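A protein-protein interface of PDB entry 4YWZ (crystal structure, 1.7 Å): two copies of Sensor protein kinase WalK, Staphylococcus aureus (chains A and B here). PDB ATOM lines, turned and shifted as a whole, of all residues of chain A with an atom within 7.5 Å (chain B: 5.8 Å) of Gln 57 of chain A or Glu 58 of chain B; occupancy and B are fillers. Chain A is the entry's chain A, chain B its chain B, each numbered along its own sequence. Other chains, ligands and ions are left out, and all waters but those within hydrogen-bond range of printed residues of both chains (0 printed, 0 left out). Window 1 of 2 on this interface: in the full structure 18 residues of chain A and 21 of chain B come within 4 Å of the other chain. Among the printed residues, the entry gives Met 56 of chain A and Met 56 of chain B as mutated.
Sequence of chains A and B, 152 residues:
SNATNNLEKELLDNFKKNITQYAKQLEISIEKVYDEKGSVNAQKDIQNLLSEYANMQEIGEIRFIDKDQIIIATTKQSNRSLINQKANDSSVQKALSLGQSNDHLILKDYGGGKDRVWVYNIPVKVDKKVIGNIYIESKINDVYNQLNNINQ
The side-chain amide oxygen (OE1) of Gln 57 of chain A lies close to the side-chain carboxylate (OE1) of Glu 58 of chain B, at 2.9 Å. The side-chain amide nitrogen (NE2) of Gln 57 of chain A lies close to the side-chain amide nitrogen (NE2) of Gln 57 of chain B (3.4 Å). The side-chain amide oxygen (OE1) of Gln 57 of chain A sits close to the side-chain carboxylate (OD2) of Asp 142 of chain B.
The side-chain carboxylate (OD2) of Asp 142 of chain B lies close to the side-chain carboxylate (OE2) of Glu 58 of chain B, 2.5 Å away. The backbone carbonyl oxygen (O) of Glu 58 of chain B sits at hydrogen-bond distance from the backbone NH (N) of Lys 139 of chain B (2.8 Å).
Gln 57 of chain A touches three residues of chain B. Printed residues of chain A within 4 Å of Asp 142 of chain B: Gln 57 (3.1 Å). Printed residues of chain A within 4 Å of Gln 57 of chain B: Gln 57. The nearest residue of chain A that does not touch Glu 58 of chain B is Glu 58 of chain A (5.5 Å).
Gln 57 of chain B touches its own counterpart, Gln 57 of chain A. Gln 57 of chain A touches Glu 58 of chain B, but with the chains exchanged Glu 58 of chain A does not touch Gln 57 of chain B (7.6 Å). Gln 57 of chain A touches Asp 142 of chain B, but with the chains exchanged Asp 142 of chain A does not touch Gln 57 of chain B (6.1 Å). 10 positions are printed for both chains. Of the 3 pairs that touch across the chains among the printed residues, 1 has its exchanged pair printed and touching as well.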
ATOM      1  N   PHE A  15     -11.826 -20.217 -28.727  1.00  0.00           N
ATOM      2  CA  PHE A  15     -11.330 -21.604 -28.794  1.00  0.00           C
ATOM      3  C   PHE A  15     -11.467 -22.154 -30.247  1.00  0.00           C
ATOM      4  O   PHE A  15     -10.507 -22.722 -30.760  1.00  0.00           O
ATOM      5  CB  PHE A  15     -12.147 -22.474 -27.858  1.00  0.00           C
ATOM      6  CG  PHE A  15     -11.730 -23.918 -27.842  1.00  0.00           C
ATOM      7  CD1 PHE A  15     -12.268 -24.793 -28.748  1.00  0.00           C
ATOM      8  CD2 PHE A  15     -10.863 -24.419 -26.882  1.00  0.00           C
ATOM      9  CE1 PHE A  15     -11.899 -26.152 -28.769  1.00  0.00           C
ATOM     10  CE2 PHE A  15     -10.506 -25.729 -26.880  1.00  0.00           C
ATOM     11  CZ  PHE A  15     -11.012 -26.598 -27.846  1.00  0.00           C
ATOM     12  N   ILE A  19      -8.497 -23.323 -33.162  1.00  0.00           N
ATOM     13  CA  ILE A  19      -8.474 -24.628 -33.793  1.00  0.00           C
ATOM     14  C   ILE A  19      -8.526 -24.395 -35.337  1.00  0.00           C
ATOM     15  O   ILE A  19      -7.808 -25.070 -36.058  1.00  0.00           O
ATOM     16  CB  ILE A  19      -9.638 -25.488 -33.359  1.00  0.00           C
ATOM     17  CG1 ILE A  19      -9.576 -25.905 -31.862  1.00  0.00           C
ATOM     18  CG2 ILE A  19      -9.755 -26.730 -34.217  1.00  0.00           C
ATOM     19  CD1 ILE A  19      -8.300 -26.515 -31.424  1.00  0.00           C
ATOM     20  N   TYR A  53       0.732 -31.342 -35.284  1.00  0.00           N
ATOM     21  CA  TYR A  53      -0.387 -30.554 -34.948  1.00  0.00           C
ATOM     22  C   TYR A  53      -1.190 -31.014 -33.694  1.00  0.00           C
ATOM     23  O   TYR A  53      -1.756 -30.126 -32.955  1.00  0.00           O
ATOM     24  CB  TYR A  53      -1.304 -30.335 -36.207  1.00  0.00           C
ATOM     25  CG  TYR A  53      -0.747 -29.294 -37.160  1.00  0.00           C
ATOM     26  CD1 TYR A  53      -1.291 -28.049 -37.222  1.00  0.00           C
ATOM     27  CD2 TYR A  53       0.287 -29.575 -37.989  1.00  0.00           C
ATOM     28  CE1 TYR A  53      -0.767 -27.051 -38.054  1.00  0.00           C
ATOM     29  CE2 TYR A  53       0.818 -28.591 -38.802  1.00  0.00           C
ATOM     30  CZ  TYR A  53       0.240 -27.377 -38.855  1.00  0.00           C
ATOM     31  OH  TYR A  53       0.751 -26.430 -39.716  1.00  0.00           O
ATOM     32  N   ALA A  54      -1.273 -32.323 -33.536  1.00  0.00           N
ATOM     33  CA  ALA A  54      -2.105 -32.894 -32.485  1.00  0.00           C
ATOM     34  C   ALA A  54      -1.409 -32.744 -31.142  1.00  0.00           C
ATOM     35  O   ALA A  54      -2.045 -32.954 -30.110  1.00  0.00           O
ATOM     36  CB  ALA A  54      -2.451 -34.352 -32.735  1.00  0.00           C
ATOM     37  N   ASN A  55      -0.165 -32.333 -31.170  1.00  0.00           N
ATOM     38  CA  ASN A  55       0.532 -32.049 -29.884  1.00  0.00           C
ATOM     39  C   ASN A  55      -0.078 -30.904 -29.143  1.00  0.00           C
ATOM     40  O   ASN A  55       0.167 -30.742 -27.941  1.00  0.00           O
ATOM     41  CB  ASN A  55       1.981 -31.673 -30.180  1.00  0.00           C
ATOM     42  CG  ASN A  55       2.855 -31.841 -28.985  1.00  0.00           C
ATOM     43  OD1 ASN A  55       3.399 -30.863 -28.452  1.00  0.00           O
ATOM     44  ND2 ASN A  55       2.976 -33.099 -28.525  1.00  0.00           N
ATOM     45  N   MET A  56      -0.822 -30.028 -29.825  1.00  0.00           N
ATOM     46  CA  MET A  56      -1.421 -28.912 -29.169  1.00  0.00           C
ATOM     47  C   MET A  56      -2.323 -29.475 -28.061  1.00  0.00           C
ATOM     48  O   MET A  56      -2.980 -30.528 -28.233  1.00  0.00           O
ATOM     49  CB  MET A  56      -2.149 -28.098 -30.220  1.00  0.00           C
ATOM     50  CG  MET A  56      -3.212 -27.196 -29.730  1.00  0.00           C
ATOM     51  SD  MET A  56      -3.884 -26.561 -31.465  1.00  0.00           S
ATOM     52  CE  MET A  56      -4.886 -25.309 -30.467  1.00  0.00           C
ATOM     53  N   GLN A  57      -2.341 -28.784 -26.912  1.00  0.00           N
ATOM     54  CA  GLN A  57      -3.148 -29.282 -25.764  1.00  0.00           C
ATOM     55  C   GLN A  57      -4.663 -29.400 -26.088  1.00  0.00           C
ATOM     56  O   GLN A  57      -5.322 -30.267 -25.568  1.00  0.00           O
ATOM     57  CB  GLN A  57      -2.977 -28.443 -24.481  1.00  0.00           C
ATOM     58  CG  GLN A  57      -1.625 -27.717 -24.329  1.00  0.00           C
ATOM     59  CD  GLN A  57      -1.668 -26.559 -23.258  1.00  0.00           C
ATOM     60  OE1 GLN A  57      -1.302 -25.417 -23.543  1.00  0.00           O
ATOM     61  NE2 GLN A  57      -2.148 -26.871 -22.044  1.00  0.00           N
ATOM     62  N   GLU A  58      -5.171 -28.486 -26.851  1.00  0.00           N
ATOM     63  CA  GLU A  58      -6.607 -28.426 -27.136  1.00  0.00           C
ATOM     64  C   GLU A  58      -7.085 -29.497 -28.147  1.00  0.00           C
ATOM     65  O   GLU A  58      -8.290 -29.603 -28.343  1.00  0.00           O
ATOM     66  CB  GLU A  58      -6.986 -27.044 -27.619  1.00  0.00           C
ATOM     67  CG  GLU A  58      -6.692 -25.884 -26.620  1.00  0.00           C
ATOM     68  CD  GLU A  58      -5.334 -25.165 -26.780  1.00  0.00           C
ATOM     69  OE1 GLU A  58      -4.291 -25.816 -27.151  1.00  0.00           O
ATOM     70  OE2 GLU A  58      -5.320 -23.915 -26.497  1.00  0.00           O
ATOM     71  N   ILE A  59      -6.159 -30.190 -28.855  1.00  0.00           N
ATOM     72  CA  ILE A  59      -6.585 -31.209 -29.836  1.00  0.00           C
ATOM     73  C   ILE A  59      -6.518 -32.593 -29.222  1.00  0.00           C
ATOM     74  O   ILE A  59      -5.463 -33.028 -28.649  1.00  0.00           O
ATOM     75  CB  ILE A  59      -5.742 -31.085 -31.089  1.00  0.00           C
ATOM     76  CG1 ILE A  59      -6.200 -29.804 -31.810  1.00  0.00           C
ATOM     77  CG2 ILE A  59      -5.971 -32.345 -31.984  1.00  0.00           C
ATOM     78  CD1 ILE A  59      -5.588 -29.540 -33.133  1.00  0.00           C
ATOM     79  N   GLY A  60      -7.638 -33.323 -29.288  1.00  0.00           N
ATOM     80  CA  GLY A  60      -7.750 -34.714 -28.867  1.00  0.00           C
ATOM     81  C   GLY A  60      -7.170 -35.701 -29.868  1.00  0.00           C
ATOM     82  O   GLY A  60      -6.297 -36.496 -29.566  1.00  0.00           O
ATOM     83  N   SER A 138     -11.629 -31.802 -30.747  1.00  0.00           N
ATOM     84  CA  SER A 138     -10.968 -30.790 -29.914  1.00  0.00           C
ATOM     85  C   SER A 138     -11.649 -30.713 -28.578  1.00  0.00           C
ATOM     86  O   SER A 138     -12.872 -30.881 -28.419  1.00  0.00           O
ATOM     87  CB  SER A 138     -10.878 -29.490 -30.698  1.00  0.00           C
ATOM     88  OG  SER A 138     -12.110 -28.915 -30.854  1.00  0.00           O
ATOM     89  N   LYS A 139     -10.815 -30.394 -27.576  1.00  0.00           N
ATOM     90  CA  LYS A 139     -11.225 -30.469 -26.157  1.00  0.00           C
ATOM     91  C   LYS A 139     -11.917 -29.216 -25.679  1.00  0.00           C
ATOM     92  O   LYS A 139     -11.519 -28.529 -24.684  1.00  0.00           O
ATOM     93  CB  LYS A 139      -9.989 -30.764 -25.343  1.00  0.00           C
ATOM     94  CG  LYS A 139      -9.288 -32.070 -25.620  1.00  0.00           C
ATOM     95  CD  LYS A 139      -8.052 -32.230 -24.797  1.00  0.00           C
ATOM     96  CE  LYS A 139      -7.377 -33.520 -25.169  1.00  0.00           C
ATOM     97  NZ  LYS A 139      -6.142 -33.873 -24.386  1.00  0.00           N
ATOM     98  N   ASP A 142     -12.732 -28.135 -21.978  1.00  0.00           N
ATOM     99  CA  ASP A 142     -11.897 -27.359 -21.108  1.00  0.00           C
ATOM    100  C   ASP A 142     -12.426 -25.937 -20.906  1.00  0.00           C
ATOM    101  O   ASP A 142     -12.229 -25.394 -19.795  1.00  0.00           O
ATOM    102  CB  ASP A 142     -10.437 -27.344 -21.612  1.00  0.00           C
ATOM    103  CG  ASP A 142      -9.634 -28.712 -21.434  1.00  0.00           C
ATOM    104  OD1 ASP A 142      -9.935 -29.565 -20.539  1.00  0.00           O
ATOM    105  OD2 ASP A 142      -8.581 -28.758 -22.141  1.00  0.00           O
ATOM    106  N   PHE B  15      -4.327 -16.036 -27.988  1.00  0.00           N
ATOM    107  CA  PHE B  15      -3.987 -16.315 -26.618  1.00  0.00           C
ATOM    108  C   PHE B  15      -4.241 -15.099 -25.700  1.00  0.00           C
ATOM    109  O   PHE B  15      -4.814 -15.220 -24.596  1.00  0.00           O
ATOM    110  CB  PHE B  15      -2.503 -16.708 -26.610  1.00  0.00           C
ATOM    111  CG  PHE B  15      -1.974 -17.026 -25.232  1.00  0.00           C
ATOM    112  CD1 PHE B  15      -1.493 -16.022 -24.460  1.00  0.00           C
ATOM    113  CD2 PHE B  15      -1.929 -18.352 -24.766  1.00  0.00           C
ATOM    114  CE1 PHE B  15      -1.061 -16.305 -23.163  1.00  0.00           C
ATOM    115  CE2 PHE B  15      -1.461 -18.652 -23.521  1.00  0.00           C
ATOM    116  CZ  PHE B  15      -1.057 -17.613 -22.701  1.00  0.00           C
ATOM    117  N   ILE B  19      -6.919 -14.384 -22.366  1.00  0.00           N
ATOM    118  CA  ILE B  19      -6.465 -13.879 -21.055  1.00  0.00           C
ATOM    119  C   ILE B  19      -7.182 -12.578 -20.677  1.00  0.00           C
ATOM    120  O   ILE B  19      -7.621 -12.408 -19.549  1.00  0.00           O
ATOM    121  CB  ILE B  19      -4.938 -13.624 -21.003  1.00  0.00           C
ATOM    122  CG1 ILE B  19      -4.065 -14.878 -21.211  1.00  0.00           C
ATOM    123  CG2 ILE B  19      -4.519 -13.059 -19.673  1.00  0.00           C
ATOM    124  CD1 ILE B  19      -4.358 -16.093 -20.387  1.00  0.00           C
ATOM    125  N   MET B  56      -7.272 -21.936 -14.735  1.00  0.00           N
ATOM    126  CA  MET B  56      -7.143 -22.088 -16.166  1.00  0.00           C
ATOM    127  C   MET B  56      -5.704 -22.416 -16.519  1.00  0.00           C
ATOM    128  O   MET B  56      -4.739 -21.909 -15.919  1.00  0.00           O
ATOM    129  CB  MET B  56      -7.734 -20.940 -16.949  1.00  0.00           C
ATOM    130  CG  MET B  56      -7.273 -19.525 -16.686  1.00  0.00           C
ATOM    131  SD  MET B  56      -7.634 -18.547 -18.372  1.00  0.00           S
ATOM    132  CE  MET B  56      -6.767 -19.795 -19.589  1.00  0.00           C
ATOM    133  N   GLN B  57      -5.577 -23.260 -17.536  1.00  0.00           N
ATOM    134  CA  GLN B  57      -4.322 -23.831 -17.882  1.00  0.00           C
ATOM    135  C   GLN B  57      -3.279 -22.777 -18.254  1.00  0.00           C
ATOM    136  O   GLN B  57      -2.104 -22.939 -17.945  1.00  0.00           O
ATOM    137  CB  GLN B  57      -4.473 -24.837 -19.047  1.00  0.00           C
ATOM    138  CG  GLN B  57      -4.232 -26.304 -18.667  1.00  0.00           C
ATOM    139  CD  GLN B  57      -2.754 -26.735 -18.671  1.00  0.00           C
ATOM    140  OE1 GLN B  57      -1.840 -25.912 -18.533  1.00  0.00           O
ATOM    141  NE2 GLN B  57      -2.520 -28.046 -18.846  1.00  0.00           N
ATOM    142  N   GLU B  58      -3.756 -21.751 -18.912  1.00  0.00           N
ATOM    143  CA  GLU B  58      -2.837 -20.762 -19.500  1.00  0.00           C
ATOM    144  C   GLU B  58      -2.386 -19.681 -18.492  1.00  0.00           C
ATOM    145  O   GLU B  58      -1.564 -18.889 -18.828  1.00  0.00           O
ATOM    146  CB  GLU B  58      -3.438 -20.163 -20.740  1.00  0.00           C
ATOM    147  CG  GLU B  58      -3.491 -21.224 -21.883  1.00  0.00           C
ATOM    148  CD  GLU B  58      -2.223 -22.164 -21.978  1.00  0.00           C
ATOM    149  OE1 GLU B  58      -2.459 -23.428 -21.806  1.00  0.00           O
ATOM    150  OE2 GLU B  58      -0.978 -21.754 -22.197  1.00  0.00           O
ATOM    151  N   ILE B  59      -2.879 -19.698 -17.276  1.00  0.00           N
ATOM    152  CA  ILE B  59      -2.459 -18.686 -16.279  1.00  0.00           C
ATOM    153  C   ILE B  59      -1.495 -19.317 -15.292  1.00  0.00           C
ATOM    154  O   ILE B  59      -1.765 -20.387 -14.716  1.00  0.00           O
ATOM    155  CB  ILE B  59      -3.651 -18.071 -15.543  1.00  0.00           C
ATOM    156  CG1 ILE B  59      -4.417 -17.122 -16.498  1.00  0.00           C
ATOM    157  CG2 ILE B  59      -3.149 -17.374 -14.206  1.00  0.00           C
ATOM    158  CD1 ILE B  59      -5.581 -16.403 -15.929  1.00  0.00           C
ATOM    159  N   GLY B  60      -0.319 -18.722 -15.140  1.00  0.00           N
ATOM    160  CA  GLY B  60       0.742 -19.135 -14.180  1.00  0.00           C
ATOM    161  C   GLY B  60       0.416 -18.669 -12.763  1.00  0.00           C
ATOM    162  O   GLY B  60       0.281 -19.470 -11.835  1.00  0.00           O
ATOM    163  N   GLU B 137       0.690 -13.364 -14.723  1.00  0.00           N
ATOM    164  CA  GLU B 137       1.724 -14.065 -15.535  1.00  0.00           C
ATOM    165  C   GLU B 137       0.985 -15.168 -16.285  1.00  0.00           C
ATOM    166  O   GLU B 137       0.360 -16.054 -15.659  1.00  0.00           O
ATOM    167  CB  GLU B 137       2.880 -14.628 -14.679  1.00  0.00           C
ATOM    168  CG  GLU B 137       3.734 -13.523 -14.101  1.00  0.00           C
ATOM    169  CD  GLU B 137       4.872 -14.060 -13.186  1.00  0.00           C
ATOM    170  OE1 GLU B 137       5.145 -15.267 -13.241  1.00  0.00           O
ATOM    171  OE2 GLU B 137       5.408 -13.228 -12.452  1.00  0.00           O
ATOM    172  N   SER B 138       1.102 -15.184 -17.599  1.00  0.00           N
ATOM    173  CA  SER B 138       0.442 -16.169 -18.455  1.00  0.00           C
ATOM    174  C   SER B 138       1.403 -16.899 -19.308  1.00  0.00           C
ATOM    175  O   SER B 138       2.462 -16.376 -19.742  1.00  0.00           O
ATOM    176  CB  SER B 138      -0.725 -15.489 -19.226  1.00  0.00           C
ATOM    177  OG  SER B 138      -0.225 -14.600 -20.167  1.00  0.00           O
ATOM    178  N   LYS B 139       1.028 -18.175 -19.552  1.00  0.00           N
ATOM    179  CA  LYS B 139       1.957 -19.155 -20.166  1.00  0.00           C
ATOM    180  C   LYS B 139       2.017 -19.083 -21.687  1.00  0.00           C
ATOM    181  O   LYS B 139       1.763 -20.055 -22.414  1.00  0.00           O
ATOM    182  CB  LYS B 139       1.591 -20.531 -19.689  1.00  0.00           C
ATOM    183  CG  LYS B 139       1.701 -20.652 -18.219  1.00  0.00           C
ATOM    184  CD  LYS B 139       1.350 -22.096 -17.833  1.00  0.00           C
ATOM    185  CE  LYS B 139       1.314 -22.262 -16.364  1.00  0.00           C
ATOM    186  NZ  LYS B 139       0.934 -23.666 -15.891  1.00  0.00           N
ATOM    187  N   ILE B 140       2.350 -17.896 -22.215  1.00  0.00           N
ATOM    188  CA  ILE B 140       2.392 -17.713 -23.644  1.00  0.00           C
ATOM    189  C   ILE B 140       3.437 -18.594 -24.359  1.00  0.00           C
ATOM    190  O   ILE B 140       3.360 -18.780 -25.568  1.00  0.00           O
ATOM    191  CB  ILE B 140       2.640 -16.214 -24.028  1.00  0.00           C
ATOM    192  CG1 ILE B 140       2.026 -15.912 -25.392  1.00  0.00           C
ATOM    193  CG2 ILE B 140       4.066 -15.751 -23.838  1.00  0.00           C
ATOM    194  CD1 ILE B 140       1.944 -14.450 -25.616  1.00  0.00           C
ATOM    195  N   ASP B 142       3.526 -21.598 -24.284  1.00  0.00           N
ATOM    196  CA  ASP B 142       2.788 -22.707 -24.878  1.00  0.00           C
ATOM    197  C   ASP B 142       2.539 -22.427 -26.368  1.00  0.00           C
ATOM    198  O   ASP B 142       2.574 -23.392 -27.160  1.00  0.00           O
ATOM    199  CB  ASP B 142       1.465 -22.967 -24.136  1.00  0.00           C
ATOM    200  CG  ASP B 142       1.663 -23.661 -22.765  1.00  0.00           C
ATOM    201  OD1 ASP B 142       2.709 -24.322 -22.531  1.00  0.00           O
ATOM    202  OD2 ASP B 142       0.695 -23.590 -21.980  1.00  0.00           O
ATOM    203  N   VAL B 143       2.253 -21.170 -26.797  1.00  0.00           N
ATOM    204  CA  VAL B 143       2.060 -20.830 -28.178  1.00  0.00           C
ATOM    205  C   VAL B 143       3.387 -20.961 -29.002  1.00  0.00           C
ATOM    206  O   VAL B 143       3.461 -21.567 -30.021  1.00  0.00           O
ATOM    207  CB  VAL B 143       1.466 -19.459 -28.346  1.00  0.00           C
ATOM    208  CG1 VAL B 143       1.278 -19.179 -29.805  1.00  0.00           C
ATOM    209  CG2 VAL B 143       0.212 -19.305 -27.444  1.00  0.00           C
